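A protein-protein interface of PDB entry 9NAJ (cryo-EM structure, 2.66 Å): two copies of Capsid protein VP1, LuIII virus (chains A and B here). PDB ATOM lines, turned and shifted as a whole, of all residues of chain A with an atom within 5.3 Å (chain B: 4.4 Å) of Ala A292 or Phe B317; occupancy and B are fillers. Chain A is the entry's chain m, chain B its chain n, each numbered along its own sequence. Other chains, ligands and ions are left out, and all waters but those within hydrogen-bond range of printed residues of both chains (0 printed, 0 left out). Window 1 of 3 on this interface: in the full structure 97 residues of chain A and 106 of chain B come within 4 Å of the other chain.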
ATOM      1  N   THR A 248     -29.194   5.589  -0.496  1.00  0.00           N
ATOM      2  CA  THR A 248     -28.137   6.469  -0.031  1.00  0.00           C
ATOM      3  C   THR A 248     -27.724   7.398  -1.166  1.00  0.00           C
ATOM      4  O   THR A 248     -28.181   7.272  -2.302  1.00  0.00           O
ATOM      5  CB  THR A 248     -26.981   5.615   0.493  1.00  0.00           C
ATOM      6  OG1 THR A 248     -27.458   4.790   1.555  1.00  0.00           O
ATOM      7  CG2 THR A 248     -25.851   6.429   1.037  1.00  0.00           C
ATOM      8  N   ASN A 249     -26.827   8.334  -0.875  1.00  0.00           N
ATOM      9  CA  ASN A 249     -26.348   9.231  -1.908  1.00  0.00           C
ATOM     10  C   ASN A 249     -25.540   8.493  -2.952  1.00  0.00           C
ATOM     11  O   ASN A 249     -25.324   9.014  -4.046  1.00  0.00           O
ATOM     12  CB  ASN A 249     -25.513  10.340  -1.290  1.00  0.00           C
ATOM     13  CG  ASN A 249     -25.268  11.455  -2.248  1.00  0.00           C
ATOM     14  OD1 ASN A 249     -26.083  11.709  -3.120  1.00  0.00           O
ATOM     15  ND2 ASN A 249     -24.149  12.132  -2.106  1.00  0.00           N
ATOM     16  N   ARG A 250     -25.090   7.295  -2.643  1.00  0.00           N
ATOM     17  CA  ARG A 250     -24.319   6.512  -3.581  1.00  0.00           C
ATOM     18  C   ARG A 250     -25.186   5.514  -4.339  1.00  0.00           C
ATOM     19  O   ARG A 250     -24.688   4.801  -5.210  1.00  0.00           O
ATOM     20  CB  ARG A 250     -23.183   5.837  -2.818  1.00  0.00           C
ATOM     21  CG  ARG A 250     -22.201   5.114  -3.650  1.00  0.00           C
ATOM     22  CD  ARG A 250     -21.081   4.634  -2.809  1.00  0.00           C
ATOM     23  NE  ARG A 250     -20.155   3.865  -3.609  1.00  0.00           N
ATOM     24  CZ  ARG A 250     -18.985   3.439  -3.172  1.00  0.00           C
ATOM     25  NH1 ARG A 250     -18.596   3.716  -1.943  1.00  0.00           N
ATOM     26  NH2 ARG A 250     -18.207   2.730  -3.965  1.00  0.00           N
ATOM     27  N   THR A 290     -15.268   7.234 -10.630  1.00  0.00           N
ATOM     28  CA  THR A 290     -15.491   6.168  -9.675  1.00  0.00           C
ATOM     29  C   THR A 290     -16.853   6.356  -9.049  1.00  0.00           C
ATOM     30  O   THR A 290     -17.407   7.455  -9.041  1.00  0.00           O
ATOM     31  CB  THR A 290     -14.425   6.139  -8.597  1.00  0.00           C
ATOM     32  OG1 THR A 290     -14.445   7.373  -7.877  1.00  0.00           O
ATOM     33  CG2 THR A 290     -13.070   5.967  -9.227  1.00  0.00           C
ATOM     34  N   GLU A 291     -17.390   5.261  -8.531  1.00  0.00           N
ATOM     35  CA  GLU A 291     -18.716   5.309  -7.947  1.00  0.00           C
ATOM     36  C   GLU A 291     -18.749   6.262  -6.766  1.00  0.00           C
ATOM     37  O   GLU A 291     -19.791   6.849  -6.467  1.00  0.00           O
ATOM     38  CB  GLU A 291     -19.124   3.903  -7.534  1.00  0.00           C
ATOM     39  CG  GLU A 291     -20.552   3.752  -7.115  1.00  0.00           C
ATOM     40  CD  GLU A 291     -21.496   3.951  -8.272  1.00  0.00           C
ATOM     41  OE1 GLU A 291     -21.032   3.960  -9.427  1.00  0.00           O
ATOM     42  OE2 GLU A 291     -22.710   4.093  -8.029  1.00  0.00           O
ATOM     43  N   ALA A 292     -17.612   6.441  -6.101  1.00  0.00           N
ATOM     44  CA  ALA A 292     -17.532   7.340  -4.958  1.00  0.00           C
ATOM     45  C   ALA A 292     -17.400   8.794  -5.380  1.00  0.00           C
ATOM     46  O   ALA A 292     -17.940   9.682  -4.718  1.00  0.00           O
ATOM     47  CB  ALA A 292     -16.358   6.944  -4.070  1.00  0.00           C
ATOM     48  N   THR A 293     -16.672   9.065  -6.455  1.00  0.00           N
ATOM     49  CA  THR A 293     -16.384  10.434  -6.844  1.00  0.00           C
ATOM     50  C   THR A 293     -17.327  10.990  -7.897  1.00  0.00           C
ATOM     51  O   THR A 293     -17.196  12.158  -8.259  1.00  0.00           O
ATOM     52  CB  THR A 293     -14.951  10.542  -7.350  1.00  0.00           C
ATOM     53  OG1 THR A 293     -14.769   9.647  -8.448  1.00  0.00           O
ATOM     54  CG2 THR A 293     -13.983  10.194  -6.255  1.00  0.00           C
ATOM     55  N   ARG A 294     -18.269  10.203  -8.396  1.00  0.00           N
ATOM     56  CA  ARG A 294     -19.160  10.717  -9.423  1.00  0.00           C
ATOM     57  C   ARG A 294     -20.196  11.654  -8.822  1.00  0.00           C
ATOM     58  O   ARG A 294     -20.604  11.512  -7.671  1.00  0.00           O
ATOM     59  CB  ARG A 294     -19.850   9.574 -10.157  1.00  0.00           C
ATOM     60  CG  ARG A 294     -20.638   8.697  -9.250  1.00  0.00           C
ATOM     61  CD  ARG A 294     -21.325   7.584  -9.986  1.00  0.00           C
ATOM     62  NE  ARG A 294     -22.395   8.061 -10.846  1.00  0.00           N
ATOM     63  CZ  ARG A 294     -23.123   7.266 -11.616  1.00  0.00           C
ATOM     64  NH1 ARG A 294     -22.889   5.967 -11.624  1.00  0.00           N
ATOM     65  NH2 ARG A 294     -24.089   7.765 -12.364  1.00  0.00           N
ATOM     66  N   GLN A 299     -27.113  16.041  -1.934  1.00  0.00           N
ATOM     67  CA  GLN A 299     -26.587  15.438  -0.721  1.00  0.00           C
ATOM     68  C   GLN A 299     -27.741  14.845   0.072  1.00  0.00           C
ATOM     69  O   GLN A 299     -28.642  15.572   0.493  1.00  0.00           O
ATOM     70  CB  GLN A 299     -25.871  16.470   0.139  1.00  0.00           C
ATOM     71  CG  GLN A 299     -25.202  15.868   1.339  1.00  0.00           C
ATOM     72  CD  GLN A 299     -24.503  16.892   2.186  1.00  0.00           C
ATOM     73  OE1 GLN A 299     -24.482  18.071   1.858  1.00  0.00           O
ATOM     74  NE2 GLN A 299     -23.919  16.448   3.284  1.00  0.00           N
ATOM     75  N   VAL A 300     -27.707  13.541   0.299  1.00  0.00           N
ATOM     76  CA  VAL A 300     -28.723  12.876   1.101  1.00  0.00           C
ATOM     77  C   VAL A 300     -28.197  12.761   2.521  1.00  0.00           C
ATOM     78  O   VAL A 300     -27.203  12.071   2.768  1.00  0.00           O
ATOM     79  CB  VAL A 300     -29.085  11.502   0.528  1.00  0.00           C
ATOM     80  CG1 VAL A 300     -30.055  10.809   1.442  1.00  0.00           C
ATOM     81  CG2 VAL A 300     -29.680  11.662  -0.845  1.00  0.00           C
ATOM     82  N   ARG A 370     -25.158   9.207   8.976  1.00  0.00           N
ATOM     83  CA  ARG A 370     -23.726   9.419   8.805  1.00  0.00           C
ATOM     84  C   ARG A 370     -22.961   8.514   9.746  1.00  0.00           C
ATOM     85  O   ARG A 370     -23.236   8.496  10.947  1.00  0.00           O
ATOM     86  CB  ARG A 370     -23.306  10.857   9.090  1.00  0.00           C
ATOM     87  CG  ARG A 370     -23.945  11.860   8.210  1.00  0.00           C
ATOM     88  CD  ARG A 370     -23.601  11.549   6.801  1.00  0.00           C
ATOM     89  NE  ARG A 370     -24.179  12.506   5.883  1.00  0.00           N
ATOM     90  CZ  ARG A 370     -24.327  12.261   4.595  1.00  0.00           C
ATOM     91  NH1 ARG A 370     -23.975  11.084   4.128  1.00  0.00           N
ATOM     92  NH2 ARG A 370     -24.844  13.169   3.789  1.00  0.00           N
ATOM     93  N   ALA B  63     -11.223   6.563  -2.310  1.00  0.00           N
ATOM     94  CA  ALA B  63     -11.988   7.366  -3.253  1.00  0.00           C
ATOM     95  C   ALA B  63     -12.280   6.637  -4.553  1.00  0.00           C
ATOM     96  O   ALA B  63     -13.144   7.082  -5.311  1.00  0.00           O
ATOM     97  CB  ALA B  63     -11.254   8.668  -3.550  1.00  0.00           C
ATOM     98  N   ASP B  65     -13.384   3.483  -4.656  1.00  0.00           N
ATOM     99  CA  ASP B  65     -14.310   2.386  -4.417  1.00  0.00           C
ATOM    100  C   ASP B  65     -15.483   2.431  -5.386  1.00  0.00           C
ATOM    101  O   ASP B  65     -16.186   3.436  -5.481  1.00  0.00           O
ATOM    102  CB  ASP B  65     -14.814   2.454  -2.980  1.00  0.00           C
ATOM    103  CG  ASP B  65     -15.775   1.346  -2.647  1.00  0.00           C
ATOM    104  OD1 ASP B  65     -15.366   0.172  -2.660  1.00  0.00           O
ATOM    105  OD2 ASP B  65     -16.938   1.645  -2.342  1.00  0.00           O
ATOM    106  N   ASN B 308     -14.990  16.843   0.306  1.00  0.00           N
ATOM    107  CA  ASN B 308     -15.645  16.265   1.467  1.00  0.00           C
ATOM    108  C   ASN B 308     -16.207  14.899   1.103  1.00  0.00           C
ATOM    109  O   ASN B 308     -17.008  14.782   0.174  1.00  0.00           O
ATOM    110  CB  ASN B 308     -16.756  17.190   1.947  1.00  0.00           C
ATOM    111  CG  ASN B 308     -17.386  16.726   3.223  1.00  0.00           C
ATOM    112  OD1 ASN B 308     -16.747  16.082   4.047  1.00  0.00           O
ATOM    113  ND2 ASN B 308     -18.657  17.048   3.398  1.00  0.00           N
ATOM    114  N   PHE B 309     -15.788  13.873   1.832  1.00  0.00           N
ATOM    115  CA  PHE B 309     -16.290  12.519   1.655  1.00  0.00           C
ATOM    116  C   PHE B 309     -17.024  12.080   2.909  1.00  0.00           C
ATOM    117  O   PHE B 309     -16.418  11.950   3.974  1.00  0.00           O
ATOM    118  CB  PHE B 309     -15.157  11.552   1.338  1.00  0.00           C
ATOM    119  CG  PHE B 309     -14.556  11.754  -0.007  1.00  0.00           C
ATOM    120  CD1 PHE B 309     -15.088  11.127  -1.109  1.00  0.00           C
ATOM    121  CD2 PHE B 309     -13.481  12.591  -0.179  1.00  0.00           C
ATOM    122  CE1 PHE B 309     -14.543  11.309  -2.344  1.00  0.00           C
ATOM    123  CE2 PHE B 309     -12.938  12.778  -1.417  1.00  0.00           C
ATOM    124  CZ  PHE B 309     -13.468  12.140  -2.498  1.00  0.00           C
ATOM    125  N   GLU B 310     -18.319  11.838   2.773  1.00  0.00           N
ATOM    126  CA  GLU B 310     -19.150  11.374   3.868  1.00  0.00           C
ATOM    127  C   GLU B 310     -19.585   9.944   3.598  1.00  0.00           C
ATOM    128  O   GLU B 310     -19.708   9.524   2.446  1.00  0.00           O
ATOM    129  CB  GLU B 310     -20.369  12.272   4.044  1.00  0.00           C
ATOM    130  CG  GLU B 310     -19.996  13.673   4.455  1.00  0.00           C
ATOM    131  CD  GLU B 310     -21.187  14.591   4.581  1.00  0.00           C
ATOM    132  OE1 GLU B 310     -22.300  14.192   4.202  1.00  0.00           O
ATOM    133  OE2 GLU B 310     -21.006  15.728   5.047  1.00  0.00           O
ATOM    134  N   SER B 312     -22.404   7.048   4.474  1.00  0.00           N
ATOM    135  CA  SER B 312     -23.585   6.374   4.987  1.00  0.00           C
ATOM    136  C   SER B 312     -23.395   4.870   4.807  1.00  0.00           C
ATOM    137  O   SER B 312     -22.296   4.392   4.526  1.00  0.00           O
ATOM    138  CB  SER B 312     -24.839   6.906   4.314  1.00  0.00           C
ATOM    139  OG  SER B 312     -25.983   6.243   4.807  1.00  0.00           O
ATOM    140  N   GLY B 315     -21.331   3.413   1.555  1.00  0.00           N
ATOM    141  CA  GLY B 315     -19.917   3.579   1.345  1.00  0.00           C
ATOM    142  C   GLY B 315     -19.539   5.038   1.371  1.00  0.00           C
ATOM    143  O   GLY B 315     -20.368   5.908   1.637  1.00  0.00           O
ATOM    144  N   PRO B 316     -18.279   5.339   1.098  1.00  0.00           N
ATOM    145  CA  PRO B 316     -17.871   6.735   0.977  1.00  0.00           C
ATOM    146  C   PRO B 316     -18.337   7.334  -0.334  1.00  0.00           C
ATOM    147  O   PRO B 316     -18.432   6.659  -1.359  1.00  0.00           O
ATOM    148  CB  PRO B 316     -16.345   6.654   1.033  1.00  0.00           C
ATOM    149  CG  PRO B 316     -16.044   5.325   0.497  1.00  0.00           C
ATOM    150  CD  PRO B 316     -17.142   4.423   0.951  1.00  0.00           C
ATOM    151  N   PHE B 317     -18.641   8.623  -0.288  1.00  0.00           N
ATOM    152  CA  PHE B 317     -18.988   9.361  -1.489  1.00  0.00           C
ATOM    153  C   PHE B 317     -18.608  10.815  -1.293  1.00  0.00           C
ATOM    154  O   PHE B 317     -18.590  11.315  -0.170  1.00  0.00           O
ATOM    155  CB  PHE B 317     -20.475   9.257  -1.816  1.00  0.00           C
ATOM    156  CG  PHE B 317     -21.365   9.730  -0.716  1.00  0.00           C
ATOM    157  CD1 PHE B 317     -21.691  11.059  -0.596  1.00  0.00           C
ATOM    158  CD2 PHE B 317     -21.897   8.840   0.185  1.00  0.00           C
ATOM    159  CE1 PHE B 317     -22.503  11.489   0.412  1.00  0.00           C
ATOM    160  CE2 PHE B 317     -22.715   9.271   1.189  1.00  0.00           C
ATOM    161  CZ  PHE B 317     -23.017  10.593   1.297  1.00  0.00           C
ATOM    162  N   LYS B 318     -18.326  11.492  -2.395  1.00  0.00           N
ATOM    163  CA  LYS B 318     -18.016  12.908  -2.331  1.00  0.00           C
ATOM    164  C   LYS B 318     -19.289  13.731  -2.269  1.00  0.00           C
ATOM    165  O   LYS B 318     -20.225  13.514  -3.038  1.00  0.00           O
ATOM    166  CB  LYS B 318     -17.198  13.347  -3.535  1.00  0.00           C
ATOM    167  CG  LYS B 318     -16.861  14.804  -3.451  1.00  0.00           C
ATOM    168  CD  LYS B 318     -15.956  15.248  -4.542  1.00  0.00           C
ATOM    169  CE  LYS B 318     -15.737  16.729  -4.437  1.00  0.00           C
ATOM    170  NZ  LYS B 318     -16.975  17.457  -4.796  1.00  0.00           N
ATOM    171  N   VAL B 319     -19.319  14.684  -1.356  1.00  0.00           N
ATOM    172  CA  VAL B 319     -20.485  15.555  -1.229  1.00  0.00           C
ATOM    173  C   VAL B 319     -20.519  16.503  -2.422  1.00  0.00           C
ATOM    174  O   VAL B 319     -19.487  17.092  -2.759  1.00  0.00           O
ATOM    175  CB  VAL B 319     -20.438  16.323   0.079  1.00  0.00           C
ATOM    176  CG1 VAL B 319     -21.583  17.298   0.151  1.00  0.00           C
ATOM    177  CG2 VAL B 319     -20.503  15.363   1.227  1.00  0.00           C
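The guanidinium group (NH1) of Arg A250 is in salt-bridge range of the side-chain carboxylate (OD2) of Asp B65 (2.7 Å).
The guanidinium group (NH1) of Arg A250 lies within hydrogen-bond range of the backbone carbonyl oxygen (O) of Pro B316.
The side-chain hydroxyl (OG1) of Thr A290 lies within hydrogen-bond range of the backbone carbonyl oxygen (O) of Ala B63, 2.9 Å away.
The backbone carbonyl oxygen (O) of Asp B65 lies within hydrogen-bond range of the backbone NH (N) of Ala A292, at 3.4 Å.
The backbone NH (N) of Lys B318 lies within hydrogen-bond range of the backbone carbonyl oxygen (O) of Ala A292, at 3.0 Å.
The side-chain amide nitrogen (NE2) of Gln A299 is in hydrogen-bond range of the side-chain carboxylate (OE1) of Glu B310.
NH2 of Arg A370 lies within salt-bridge range of OE1 of Glu B310 (2.8 Å).
Printed residues of chain B within 4 Å of Thr A290: Ala B63.
Of the printed residues of chain B, Glu A291 touches Asp B65 (3.6 Å).
Ala A292 touches just these residues of chain B: Ala B63 (3.4 Å), Asp B65 (3.4 Å), Pro B316 (3.4 Å), Phe B317 (3.4 Å) and Lys B318 (3.0 Å).
Printed residues of chain B within 4 Å of Thr A293: Ala B63.
Arg A294 touches none of the printed residues of chain B.
Of the printed residues of chain A, Ala B63 touches Thr A290, Ala A292 and Thr A293.
Phe B309 touches none of the printed residues of chain A.
Of the printed residues of chain A, Ser B312 touches Thr A248.
Phe B317 touches just these residues of chain A: Asn A249, Ala A292 and Arg A370.
The nearest residue of chain A that does not touch Phe B317 is Thr A248 (4.2 Å).
The nearest printed residue of chain B that does not touch Asn A249 is Lys B318 (4.3 Å).
Of the 11 printed residues of chain B, 9 touch a printed residue of chain A.
Among the printed residues, 17 pairs touch across the chains.
Among the printed residues, Asp or Glu carboxylates within 4 Å of a Lys or Arg side-chain nitrogen of the other chain: Arg A250 with Asp B65 and Arg A370 with Glu B310.
Among the printed residues, pairs that only touch across the chains: Arg A370 with Phe B317, Asn A249 with Phe B317, Thr A293 with Ala B63, Ala A292 with Phe B317, Ala A292 with Pro B316, Ala A292 with Ala B63, Gln A299 with Val B319, Thr A248 with Ser B312, Arg A250 with Gly B315 and Glu A291 with Asp B65.
No position is printed for both chains.
Of the 17 pairs that touch across the chains among the printed residues, none has its exchanged pair printed and touching as well.
The side-chain carboxylate (OE1) of Glu A291 is in salt-bridge range of the guanidinium group (NH1) of Arg A294, 3.5 Å away.
The side-chain amide nitrogen (NE2) of Gln A299 sits close to the guanidinium group (NH2) of Arg A370 (3.4 Å).
The backbone carbonyl oxygen (O) of Val A300 lies within hydrogen-bond range of the guanidinium group (NH2) of Arg A370 (2.8 Å).
The side-chain amide nitrogen (ND2) of Asn B308 sits at hydrogen-bond distance from the side-chain carboxylate (OE2) of Glu B310, at 3.2 Å.
The backbone NH of Val B319 is in hydrogen-bond range of the backbone carbonyl oxygen of Asn B308, 2.8 Å away.
O of Phe B317 sits at hydrogen-bond distance from N of Glu B310, 3.0 Å away.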
